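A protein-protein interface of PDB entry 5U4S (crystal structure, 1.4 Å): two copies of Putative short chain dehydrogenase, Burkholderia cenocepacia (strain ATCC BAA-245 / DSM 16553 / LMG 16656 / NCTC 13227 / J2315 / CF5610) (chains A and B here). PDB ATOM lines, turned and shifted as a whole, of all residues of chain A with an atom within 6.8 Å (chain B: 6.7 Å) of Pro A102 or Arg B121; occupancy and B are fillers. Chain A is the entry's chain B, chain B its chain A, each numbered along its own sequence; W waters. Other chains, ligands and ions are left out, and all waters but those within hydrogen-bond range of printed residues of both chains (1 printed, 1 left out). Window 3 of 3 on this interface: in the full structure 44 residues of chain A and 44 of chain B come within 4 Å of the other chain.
No position is printed for both chains.
Among the printed residues, pairs that only touch across the chains: Val A96 with Leu B117, Leu A97 with Met B120, Leu A97 with Ser B124 and Ala A99 with Arg B121.
The guanidinium group (NH1) of Arg B121 lies within hydrogen-bond range of the backbone carbonyl oxygen (O) of Pro A102 (2.9 Å). The guanidinium group (NE) of Arg B121 sits at hydrogen-bond distance from the backbone carbonyl oxygen (O) of Val A96 (2.8 Å).
The backbone carbonyl oxygen (O) of Met B120 is in hydrogen-bond range of the side-chain hydroxyl (OG) of Ser B124 (2.7 Å).
Water W1 bridges OD1 of Asn B118 (2.8 Å) and NH2 of Arg A106 (3.2 Å).
Printed residues of chain A that touch a printed residue of chain B: Val A96, Leu A97, Ala A99 and Pro A102. Hydrophobic or aromatic side chains of chain B within 4 Å of the printed part of chain A: Leu B117 and Met B120. Among the printed residues, 6 pairs touch across the chains. Among the printed residues, no Asp or Glu carboxylate lies within 4 Å of a Lys or Arg side-chain nitrogen of the other chain.
Of the printed residues of chain B, Ala A99 touches Arg B121. Of chain B, only Arg B121 comes within 4 Å of Pro A102. Of the printed residues of chain A, Leu B117 touches Val A96. Asn B118 touches none of the printed residues of chain A. Printed residues of chain A within 4 Å of Met B120: Leu A97. Of the printed residues of chain A, Ser B124 touches Leu A97 (3.9 Å).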
ATOM      1  N   GLN A  94     -25.663 -15.746   5.287  1.00  0.00           N
ATOM      2  CA  GLN A  94     -26.605 -16.426   4.410  1.00  0.00           C
ATOM      3  C   GLN A  94     -27.054 -17.777   4.950  1.00  0.00           C
ATOM      4  O   GLN A  94     -26.271 -18.514   5.568  1.00  0.00           O
ATOM      5  CB  GLN A  94     -26.036 -16.566   2.987  1.00  0.00           C
ATOM      6  CG  GLN A  94     -25.755 -15.178   2.445  1.00  0.00           C
ATOM      7  CD  GLN A  94     -25.598 -15.099   0.978  1.00  0.00           C
ATOM      8  OE1 GLN A  94     -26.203 -15.858   0.246  1.00  0.00           O
ATOM      9  NE2 GLN A  94     -24.772 -14.159   0.519  1.00  0.00           N
ATOM     10  N   PRO A  95     -28.313 -18.135   4.714  1.00  0.00           N
ATOM     11  CA  PRO A  95     -28.762 -19.490   5.053  1.00  0.00           C
ATOM     12  C   PRO A  95     -28.119 -20.518   4.134  1.00  0.00           C
ATOM     13  O   PRO A  95     -27.584 -20.191   3.068  1.00  0.00           O
ATOM     14  CB  PRO A  95     -30.277 -19.416   4.836  1.00  0.00           C
ATOM     15  CG  PRO A  95     -30.461 -18.344   3.803  1.00  0.00           C
ATOM     16  CD  PRO A  95     -29.374 -17.324   4.082  1.00  0.00           C
ATOM     17  N   VAL A  96     -28.189 -21.789   4.556  1.00  0.00           N
ATOM     18  CA  VAL A  96     -27.596 -22.860   3.743  1.00  0.00           C
ATOM     19  C   VAL A  96     -28.415 -23.162   2.495  1.00  0.00           C
ATOM     20  O   VAL A  96     -27.843 -23.504   1.455  1.00  0.00           O
ATOM     21  CB  VAL A  96     -27.285 -24.132   4.556  1.00  0.00           C
ATOM     22  CG1 VAL A  96     -26.053 -23.892   5.415  1.00  0.00           C
ATOM     23  CG2 VAL A  96     -28.483 -24.575   5.398  1.00  0.00           C
ATOM     24  N   LEU A  97     -29.746 -23.107   2.575  1.00  0.00           N
ATOM     25  CA  LEU A  97     -30.548 -23.470   1.403  1.00  0.00           C
ATOM     26  C   LEU A  97     -30.894 -22.252   0.553  1.00  0.00           C
ATOM     27  O   LEU A  97     -30.503 -22.169  -0.621  1.00  0.00           O
ATOM     28  CB  LEU A  97     -31.820 -24.232   1.805  1.00  0.00           C
ATOM     29  CG  LEU A  97     -31.605 -25.506   2.620  1.00  0.00           C
ATOM     30  CD1 LEU A  97     -32.910 -26.266   2.734  1.00  0.00           C
ATOM     31  CD2 LEU A  97     -30.513 -26.399   2.008  1.00  0.00           C
ATOM     32  N   GLU A  98     -31.633 -21.305   1.120  1.00  0.00           N
ATOM     33  CA  GLU A  98     -32.082 -20.144   0.352  1.00  0.00           C
ATOM     34  C   GLU A  98     -31.013 -19.051   0.283  1.00  0.00           C
ATOM     35  O   GLU A  98     -31.285 -17.895   0.617  1.00  0.00           O
ATOM     36  CB  GLU A  98     -33.365 -19.591   0.968  1.00  0.00           C
ATOM     37  CG  GLU A  98     -34.257 -18.863  -0.031  1.00  0.00           C
ATOM     38  CD  GLU A  98     -35.561 -18.382   0.586  1.00  0.00           C
ATOM     39  OE1 GLU A  98     -36.212 -17.504  -0.020  1.00  0.00           O
ATOM     40  OE2 GLU A  98     -35.934 -18.879   1.671  1.00  0.00           O
ATOM     41  N   ALA A  99     -29.794 -19.403  -0.113  1.00  0.00           N
ATOM     42  CA  ALA A  99     -28.704 -18.436  -0.162  1.00  0.00           C
ATOM     43  C   ALA A  99     -28.781 -17.623  -1.444  1.00  0.00           C
ATOM     44  O   ALA A  99     -29.028 -18.164  -2.521  1.00  0.00           O
ATOM     45  CB  ALA A  99     -27.365 -19.165  -0.128  1.00  0.00           C
ATOM     46  N   HIS A 100     -28.577 -16.310  -1.334  1.00  0.00           N
ATOM     47  CA  HIS A 100     -28.458 -15.486  -2.537  1.00  0.00           C
ATOM     48  C   HIS A 100     -27.199 -15.838  -3.316  1.00  0.00           C
ATOM     49  O   HIS A 100     -27.217 -15.839  -4.558  1.00  0.00           O
ATOM     50  CB  HIS A 100     -28.420 -13.997  -2.174  1.00  0.00           C
ATOM     51  CG  HIS A 100     -29.764 -13.383  -1.930  1.00  0.00           C
ATOM     52  ND1 HIS A 100     -30.569 -13.742  -0.867  1.00  0.00           N
ATOM     53  CD2 HIS A 100     -30.434 -12.411  -2.598  1.00  0.00           C
ATOM     54  CE1 HIS A 100     -31.682 -13.028  -0.903  1.00  0.00           C
ATOM     55  NE2 HIS A 100     -31.624 -12.213  -1.943  1.00  0.00           N
ATOM     56  N   ASP A 101     -26.095 -16.113  -2.613  1.00  0.00           N
ATOM     57  CA  ASP A 101     -24.815 -16.510  -3.199  1.00  0.00           C
ATOM     58  C   ASP A 101     -24.553 -17.973  -2.882  1.00  0.00           C
ATOM     59  O   ASP A 101     -24.209 -18.306  -1.733  1.00  0.00           O
ATOM     60  CB  ASP A 101     -23.691 -15.646  -2.632  1.00  0.00           C
ATOM     61  CG  ASP A 101     -22.349 -15.965  -3.258  1.00  0.00           C
ATOM     62  OD1 ASP A 101     -22.268 -16.904  -4.070  1.00  0.00           O
ATOM     63  OD2 ASP A 101     -21.372 -15.250  -2.958  1.00  0.00           O
ATOM     64  N   PRO A 102     -24.720 -18.886  -3.843  1.00  0.00           N
ATOM     65  CA  PRO A 102     -24.504 -20.308  -3.543  1.00  0.00           C
ATOM     66  C   PRO A 102     -23.068 -20.632  -3.189  1.00  0.00           C
ATOM     67  O   PRO A 102     -22.821 -21.710  -2.637  1.00  0.00           O
ATOM     68  CB  PRO A 102     -24.955 -21.026  -4.823  1.00  0.00           C
ATOM     69  CG  PRO A 102     -24.826 -19.987  -5.899  1.00  0.00           C
ATOM     70  CD  PRO A 102     -25.134 -18.665  -5.235  1.00  0.00           C
ATOM     71  N   GLU A 103     -22.113 -19.735  -3.471  1.00  0.00           N
ATOM     72  CA  GLU A 103     -20.717 -19.977  -3.148  1.00  0.00           C
ATOM     73  C   GLU A 103     -20.302 -19.367  -1.825  1.00  0.00           C
ATOM     74  O   GLU A 103     -19.150 -19.523  -1.415  1.00  0.00           O
ATOM     75  CB  GLU A 103     -19.809 -19.437  -4.260  1.00  0.00           C
ATOM     76  CG  GLU A 103     -20.061 -20.120  -5.596  1.00  0.00           C
ATOM     77  CD  GLU A 103     -19.946 -21.630  -5.480  1.00  0.00           C
ATOM     78  OE1 GLU A 103     -18.939 -22.107  -4.916  1.00  0.00           O
ATOM     79  OE2 GLU A 103     -20.868 -22.340  -5.935  1.00  0.00           O
ATOM     80  N   ALA A 104     -21.214 -18.689  -1.126  1.00  0.00           N
ATOM     81  CA  ALA A 104     -20.845 -18.061   0.140  1.00  0.00           C
ATOM     82  C   ALA A 104     -20.420 -19.090   1.185  1.00  0.00           C
ATOM     83  O   ALA A 104     -19.468 -18.853   1.941  1.00  0.00           O
ATOM     84  CB  ALA A 104     -21.994 -17.206   0.661  1.00  0.00           C
ATOM     85  N   ALA A 105     -21.114 -20.236   1.254  1.00  0.00           N
ATOM     86  CA  ALA A 105     -20.758 -21.261   2.239  1.00  0.00           C
ATOM     87  C   ALA A 105     -19.324 -21.712   2.055  1.00  0.00           C
ATOM     88  O   ALA A 105     -18.582 -21.841   3.033  1.00  0.00           O
ATOM     89  CB  ALA A 105     -21.715 -22.456   2.149  1.00  0.00           C
ATOM     90  N   ARG A 106     -18.907 -21.896   0.797  1.00  0.00           N
ATOM     91  CA  ARG A 106     -17.542 -22.320   0.520  1.00  0.00           C
ATOM     92  C   ARG A 106     -16.533 -21.236   0.884  1.00  0.00           C
ATOM     93  O   ARG A 106     -15.443 -21.546   1.395  1.00  0.00           O
ATOM     94  CB  ARG A 106     -17.448 -22.727  -0.943  1.00  0.00           C
ATOM     95  CG  ARG A 106     -16.115 -23.385  -1.303  1.00  0.00           C
ATOM     96  CD  ARG A 106     -16.101 -23.842  -2.749  1.00  0.00           C
ATOM     97  NE  ARG A 106     -17.076 -24.901  -3.040  1.00  0.00           N
ATOM     98  CZ  ARG A 106     -16.826 -26.208  -2.911  1.00  0.00           C
ATOM     99  NH1 ARG A 106     -15.631 -26.621  -2.528  1.00  0.00           N
ATOM    100  NH2 ARG A 106     -17.746 -27.116  -3.210  1.00  0.00           N
ATOM    101  N   SER A 151     -24.440 -21.094   7.255  1.00  0.00           N
ATOM    102  CA  SER A 151     -23.154 -21.474   6.665  1.00  0.00           C
ATOM    103  C   SER A 151     -21.970 -20.895   7.436  1.00  0.00           C
ATOM    104  O   SER A 151     -20.908 -21.538   7.511  1.00  0.00           O
ATOM    105  CB  SER A 151     -23.085 -21.155   5.162  1.00  0.00           C
ATOM    106  OG  SER A 151     -23.368 -19.795   4.872  1.00  0.00           O
ATOM    107  N   VAL B  71     -25.798 -34.314  -9.564  1.00  0.00           N
ATOM    108  CA  VAL B  71     -26.819 -34.067  -8.557  1.00  0.00           C
ATOM    109  C   VAL B  71     -28.041 -33.404  -9.185  1.00  0.00           C
ATOM    110  O   VAL B  71     -29.183 -33.825  -8.948  1.00  0.00           O
ATOM    111  CB  VAL B  71     -26.234 -33.247  -7.399  1.00  0.00           C
ATOM    112  CG1 VAL B  71     -27.332 -32.792  -6.473  1.00  0.00           C
ATOM    113  CG2 VAL B  71     -25.218 -34.110  -6.646  1.00  0.00           C
ATOM    114  N   THR B 116     -23.323 -33.150   0.677  1.00  0.00           N
ATOM    115  CA  THR B 116     -24.630 -33.213   1.313  1.00  0.00           C
ATOM    116  C   THR B 116     -25.406 -31.926   1.071  1.00  0.00           C
ATOM    117  O   THR B 116     -26.605 -31.969   0.762  1.00  0.00           O
ATOM    118  CB  THR B 116     -24.447 -33.495   2.802  1.00  0.00           C
ATOM    119  OG1 THR B 116     -23.660 -34.692   2.946  1.00  0.00           O
ATOM    120  CG2 THR B 116     -25.797 -33.670   3.507  1.00  0.00           C
ATOM    121  N   LEU B 117     -24.727 -30.776   1.150  1.00  0.00           N
ATOM    122  CA  LEU B 117     -25.367 -29.504   0.843  1.00  0.00           C
ATOM    123  C   LEU B 117     -25.890 -29.471  -0.595  1.00  0.00           C
ATOM    124  O   LEU B 117     -27.022 -29.015  -0.836  1.00  0.00           O
ATOM    125  CB  LEU B 117     -24.381 -28.364   1.099  1.00  0.00           C
ATOM    126  CG  LEU B 117     -24.892 -26.932   0.867  1.00  0.00           C
ATOM    127  CD1 LEU B 117     -26.149 -26.672   1.721  1.00  0.00           C
ATOM    128  CD2 LEU B 117     -23.797 -25.922   1.139  1.00  0.00           C
ATOM    129  N   ASN B 118     -25.097 -29.961  -1.558  1.00  0.00           N
ATOM    130  CA  ASN B 118     -25.563 -30.017  -2.945  1.00  0.00           C
ATOM    131  C   ASN B 118     -26.864 -30.802  -3.055  1.00  0.00           C
ATOM    132  O   ASN B 118     -27.787 -30.392  -3.774  1.00  0.00           O
ATOM    133  CB  ASN B 118     -24.539 -30.721  -3.859  1.00  0.00           C
ATOM    134  CG  ASN B 118     -23.242 -29.966  -4.030  1.00  0.00           C
ATOM    135  OD1 ASN B 118     -23.167 -28.736  -3.845  1.00  0.00           O
ATOM    136  ND2 ASN B 118     -22.195 -30.710  -4.374  1.00  0.00           N
ATOM    137  N   MET B 119     -26.930 -31.949  -2.376  1.00  0.00           N
ATOM    138  CA  MET B 119     -28.115 -32.793  -2.421  1.00  0.00           C
ATOM    139  C   MET B 119     -29.310 -32.083  -1.793  1.00  0.00           C
ATOM    140  O   MET B 119     -30.421 -32.125  -2.340  1.00  0.00           O
ATOM    141  CB  MET B 119     -27.821 -34.091  -1.679  1.00  0.00           C
ATOM    142  CG  MET B 119     -26.885 -35.058  -2.413  1.00  0.00           C
ATOM    143  SD  MET B 119     -27.619 -35.773  -3.903  1.00  0.00           S
ATOM    144  CE  MET B 119     -28.997 -36.718  -3.178  1.00  0.00           C
ATOM    145  N   MET B 120     -29.104 -31.452  -0.628  1.00  0.00           N
ATOM    146  CA  MET B 120     -30.173 -30.699   0.037  1.00  0.00           C
ATOM    147  C   MET B 120     -30.734 -29.617  -0.883  1.00  0.00           C
ATOM    148  O   MET B 120     -31.955 -29.454  -1.022  1.00  0.00           O
ATOM    149  CB  MET B 120     -29.630 -30.032   1.312  1.00  0.00           C
ATOM    150  CG  MET B 120     -28.996 -30.973   2.344  1.00  0.00           C
ATOM    151  SD  MET B 120     -30.227 -31.899   3.286  1.00  0.00           S
ATOM    152  CE  MET B 120     -30.881 -30.648   4.324  1.00  0.00           C
ATOM    153  N   ARG B 121     -29.839 -28.843  -1.507  1.00  0.00           N
ATOM    154  CA  ARG B 121     -30.275 -27.736  -2.357  1.00  0.00           C
ATOM    155  C   ARG B 121     -31.051 -28.230  -3.576  1.00  0.00           C
ATOM    156  O   ARG B 121     -32.062 -27.630  -3.954  1.00  0.00           O
ATOM    157  CB  ARG B 121     -29.064 -26.905  -2.785  1.00  0.00           C
ATOM    158  CG  ARG B 121     -28.470 -26.094  -1.630  1.00  0.00           C
ATOM    159  CD  ARG B 121     -27.267 -25.310  -2.077  1.00  0.00           C
ATOM    160  NE  ARG B 121     -26.875 -24.348  -1.044  1.00  0.00           N
ATOM    161  CZ  ARG B 121     -25.808 -23.559  -1.132  1.00  0.00           C
ATOM    162  NH1 ARG B 121     -25.001 -23.607  -2.195  1.00  0.00           N
ATOM    163  NH2 ARG B 121     -25.547 -22.701  -0.146  1.00  0.00           N
ATOM    164  N   ALA B 122     -30.606 -29.329  -4.193  1.00  0.00           N
ATOM    165  CA  ALA B 122     -31.222 -29.777  -5.443  1.00  0.00           C
ATOM    166  C   ALA B 122     -32.556 -30.501  -5.241  1.00  0.00           C
ATOM    167  O   ALA B 122     -33.449 -30.386  -6.091  1.00  0.00           O
ATOM    168  CB  ALA B 122     -30.261 -30.705  -6.194  1.00  0.00           C
ATOM    169  N   PHE B 123     -32.706 -31.239  -4.131  1.00  0.00           N
ATOM    170  CA  PHE B 123     -33.874 -32.079  -3.896  1.00  0.00           C
ATOM    171  C   PHE B 123     -34.933 -31.405  -3.032  1.00  0.00           C
ATOM    172  O   PHE B 123     -36.091 -31.829  -3.060  1.00  0.00           O
ATOM    173  CB  PHE B 123     -33.425 -33.405  -3.255  1.00  0.00           C
ATOM    174  CG  PHE B 123     -32.813 -34.385  -4.231  1.00  0.00           C
ATOM    175  CD1 PHE B 123     -33.586 -35.403  -4.779  1.00  0.00           C
ATOM    176  CD2 PHE B 123     -31.476 -34.289  -4.602  1.00  0.00           C
ATOM    177  CE1 PHE B 123     -33.045 -36.298  -5.675  1.00  0.00           C
ATOM    178  CE2 PHE B 123     -30.923 -35.173  -5.514  1.00  0.00           C
ATOM    179  CZ  PHE B 123     -31.708 -36.188  -6.052  1.00  0.00           C
ATOM    180  N   SER B 124     -34.570 -30.363  -2.283  1.00  0.00           N
ATOM    181  CA  SER B 124     -35.551 -29.672  -1.447  1.00  0.00           C
ATOM    182  C   SER B 124     -36.759 -29.127  -2.199  1.00  0.00           C
ATOM    183  O   SER B 124     -37.867 -29.184  -1.639  1.00  0.00           O
ATOM    184  CB  SER B 124     -34.880 -28.563  -0.630  1.00  0.00           C
ATOM    185  OG  SER B 124     -34.218 -29.123   0.474  1.00  0.00           O
ATOM    186  N   PRO B 125     -36.634 -28.569  -3.408  1.00  0.00           N
ATOM    187  CA  PRO B 125     -37.840 -28.067  -4.088  1.00  0.00           C
ATOM    188  C   PRO B 125     -38.922 -29.118  -4.262  1.00  0.00           C
ATOM    189  O   PRO B 125     -40.101 -28.849  -3.972  1.00  0.00           O
ATOM    190  CB  PRO B 125     -37.301 -27.539  -5.426  1.00  0.00           C
ATOM    191  CG  PRO B 125     -35.898 -27.098  -5.080  1.00  0.00           C
ATOM    192  CD  PRO B 125     -35.413 -28.178  -4.153  1.00  0.00           C
HETATM  193  O   HOH W   1     -20.867 -27.185  -3.800  1.00  0.00           O
